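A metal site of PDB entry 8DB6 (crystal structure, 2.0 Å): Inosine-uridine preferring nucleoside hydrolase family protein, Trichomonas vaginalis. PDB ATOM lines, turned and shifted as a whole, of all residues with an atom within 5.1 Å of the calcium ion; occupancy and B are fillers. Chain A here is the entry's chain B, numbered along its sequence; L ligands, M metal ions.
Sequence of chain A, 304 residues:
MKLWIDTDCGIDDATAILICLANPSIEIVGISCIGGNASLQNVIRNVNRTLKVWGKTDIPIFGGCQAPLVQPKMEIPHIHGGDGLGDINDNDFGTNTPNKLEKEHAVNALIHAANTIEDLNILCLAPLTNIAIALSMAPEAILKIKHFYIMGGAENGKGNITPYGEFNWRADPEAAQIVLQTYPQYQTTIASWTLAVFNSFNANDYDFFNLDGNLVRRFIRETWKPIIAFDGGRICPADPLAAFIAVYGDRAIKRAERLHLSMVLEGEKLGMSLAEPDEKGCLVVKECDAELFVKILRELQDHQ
The side-chain amide nitrogen of Asn 168 lies close to the backbone carbonyl oxygen of Leu 125 (3.5 Å). The backbone NH (N) of Asn 37 is in hydrogen-bond range of the side-chain carboxylate (OD2) of Asp 8. OD1 of Asp 13 sits close to OD1 of Asn 37. The backbone NH (N) of Asp 239 sits at hydrogen-bond distance from the side-chain carboxylate (OD2) of Asp 12 (3.1 Å).
OD1 of Asn 37 touches the calcium ion (3.8 Å). Five residues have an atom within 4 Å of the calcium ion: Asp 8, Asp 13, Asn 37, Leu 125 and Asp 239. The nearest printed residue that does not touch the calcium ion is Asp 12 (4.3 Å).
The calcium ion is bound by O of Leu 125, OD2 of Asp 239, OD1 of Asp 13, OD1 of Asp 8, O3 of the ligand and OD2 of Asp 13. The calcium ion has six donor atoms within binding distance. Slightly farther from the calcium ion lies an oxygen (O2) of the ligand (2.9 Å).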
ATOM      1  N   ASP A   8       9.274 -18.338 -18.757  1.00  0.00           N
ATOM      2  CA  ASP A   8       7.924 -18.487 -19.303  1.00  0.00           C
ATOM      3  C   ASP A   8       7.751 -17.446 -20.408  1.00  0.00           C
ATOM      4  O   ASP A   8       6.740 -16.760 -20.450  1.00  0.00           O
ATOM      5  CB  ASP A   8       6.837 -18.372 -18.227  1.00  0.00           C
ATOM      6  CG  ASP A   8       6.845 -17.034 -17.462  1.00  0.00           C
ATOM      7  OD1 ASP A   8       7.829 -16.267 -17.547  1.00  0.00           O
ATOM      8  OD2 ASP A   8       5.840 -16.755 -16.767  1.00  0.00           O
ATOM      9  N   ASP A  12       8.558  -9.590 -21.361  1.00  0.00           N
ATOM     10  CA  ASP A  12       9.765  -9.093 -20.728  1.00  0.00           C
ATOM     11  C   ASP A  12      10.838 -10.165 -20.650  1.00  0.00           C
ATOM     12  O   ASP A  12      12.036  -9.836 -20.709  1.00  0.00           O
ATOM     13  CB  ASP A  12       9.434  -8.463 -19.363  1.00  0.00           C
ATOM     14  CG  ASP A  12       8.857  -9.432 -18.374  1.00  0.00           C
ATOM     15  OD1 ASP A  12       8.033 -10.279 -18.767  1.00  0.00           O
ATOM     16  OD2 ASP A  12       9.224  -9.322 -17.186  1.00  0.00           O
ATOM     17  N   ASP A  13      10.435 -11.461 -20.590  1.00  0.00           N
ATOM     18  CA  ASP A  13      11.425 -12.544 -20.691  1.00  0.00           C
ATOM     19  C   ASP A  13      12.260 -12.410 -21.957  1.00  0.00           C
ATOM     20  O   ASP A  13      13.487 -12.558 -21.922  1.00  0.00           O
ATOM     21  CB  ASP A  13      10.741 -13.909 -20.718  1.00  0.00           C
ATOM     22  CG  ASP A  13      10.005 -14.231 -19.457  1.00  0.00           C
ATOM     23  OD1 ASP A  13       8.937 -13.608 -19.224  1.00  0.00           O
ATOM     24  OD2 ASP A  13      10.461 -15.128 -18.688  1.00  0.00           O
ATOM     25  N   ASN A  37       3.189 -16.837 -18.121  1.00  0.00           N
ATOM     26  CA  ASN A  37       2.550 -15.859 -18.986  1.00  0.00           C
ATOM     27  C   ASN A  37       1.665 -16.521 -20.040  1.00  0.00           C
ATOM     28  O   ASN A  37       0.613 -15.976 -20.401  1.00  0.00           O
ATOM     29  CB  ASN A  37       3.623 -14.997 -19.656  1.00  0.00           C
ATOM     30  CG  ASN A  37       4.332 -14.112 -18.675  1.00  0.00           C
ATOM     31  OD1 ASN A  37       5.551 -13.898 -18.765  1.00  0.00           O
ATOM     32  ND2 ASN A  37       3.591 -13.606 -17.691  1.00  0.00           N
ATOM     33  N   LEU A 125      13.475 -16.707 -14.612  1.00  0.00           N
ATOM     34  CA  LEU A 125      12.599 -15.633 -15.033  1.00  0.00           C
ATOM     35  C   LEU A 125      11.133 -15.994 -14.891  1.00  0.00           C
ATOM     36  O   LEU A 125      10.290 -15.289 -15.446  1.00  0.00           O
ATOM     37  CB  LEU A 125      12.904 -15.238 -16.479  1.00  0.00           C
ATOM     38  CG  LEU A 125      14.331 -14.743 -16.739  1.00  0.00           C
ATOM     39  CD1 LEU A 125      14.525 -14.395 -18.219  1.00  0.00           C
ATOM     40  CD2 LEU A 125      14.657 -13.554 -15.821  1.00  0.00           C
ATOM     41  N   ALA A 126      10.790 -17.072 -14.148  1.00  0.00           N
ATOM     42  CA  ALA A 126       9.456 -17.664 -14.211  1.00  0.00           C
ATOM     43  C   ALA A 126       9.077 -18.333 -12.895  1.00  0.00           C
ATOM     44  O   ALA A 126       9.916 -18.436 -11.993  1.00  0.00           O
ATOM     45  CB  ALA A 126       9.432 -18.657 -15.382  1.00  0.00           C
ATOM     46  N   ASN A 168       5.482 -14.650 -10.252  1.00  0.00           N
ATOM     47  CA  ASN A 168       6.256 -15.890 -10.360  1.00  0.00           C
ATOM     48  C   ASN A 168       6.115 -16.719  -9.091  1.00  0.00           C
ATOM     49  O   ASN A 168       5.906 -17.937  -9.152  1.00  0.00           O
ATOM     50  CB  ASN A 168       7.732 -15.590 -10.622  1.00  0.00           C
ATOM     51  CG  ASN A 168       7.987 -15.153 -12.042  1.00  0.00           C
ATOM     52  OD1 ASN A 168       7.176 -15.376 -12.928  1.00  0.00           O
ATOM     53  ND2 ASN A 168       9.131 -14.515 -12.260  1.00  0.00           N
ATOM     54  N   ASP A 239      11.898  -8.811 -15.614  1.00  0.00           N
ATOM     55  CA  ASP A 239      12.864  -9.786 -16.137  1.00  0.00           C
ATOM     56  C   ASP A 239      14.100  -9.139 -16.769  1.00  0.00           C
ATOM     57  O   ASP A 239      15.212  -9.651 -16.526  1.00  0.00           O
ATOM     58  CB  ASP A 239      12.182 -10.722 -17.147  1.00  0.00           C
ATOM     59  CG  ASP A 239      11.304 -11.774 -16.468  1.00  0.00           C
ATOM     60  OD1 ASP A 239      11.314 -11.834 -15.227  1.00  0.00           O
ATOM     61  OD2 ASP A 239      10.599 -12.531 -17.161  1.00  0.00           O
HETATM   62  C1  LIG L   1       6.900 -11.540 -13.334  1.00  0.00           C
HETATM   63  O1  LIG L   1       6.894 -10.359 -12.575  1.00  0.00           O
HETATM   64  C2  LIG L   1       8.033 -11.482 -14.352  1.00  0.00           C
HETATM   65  O2  LIG L   1       8.796 -12.662 -14.271  1.00  0.00           O
HETATM   66  C3  LIG L   1       7.443 -11.365 -15.760  1.00  0.00           C
HETATM   67  O3  LIG L   1       6.860 -12.581 -16.131  1.00  0.00           O
HETATM   68 CA    CA M   1       8.850 -14.086 -16.851  1.00  0.00          CA
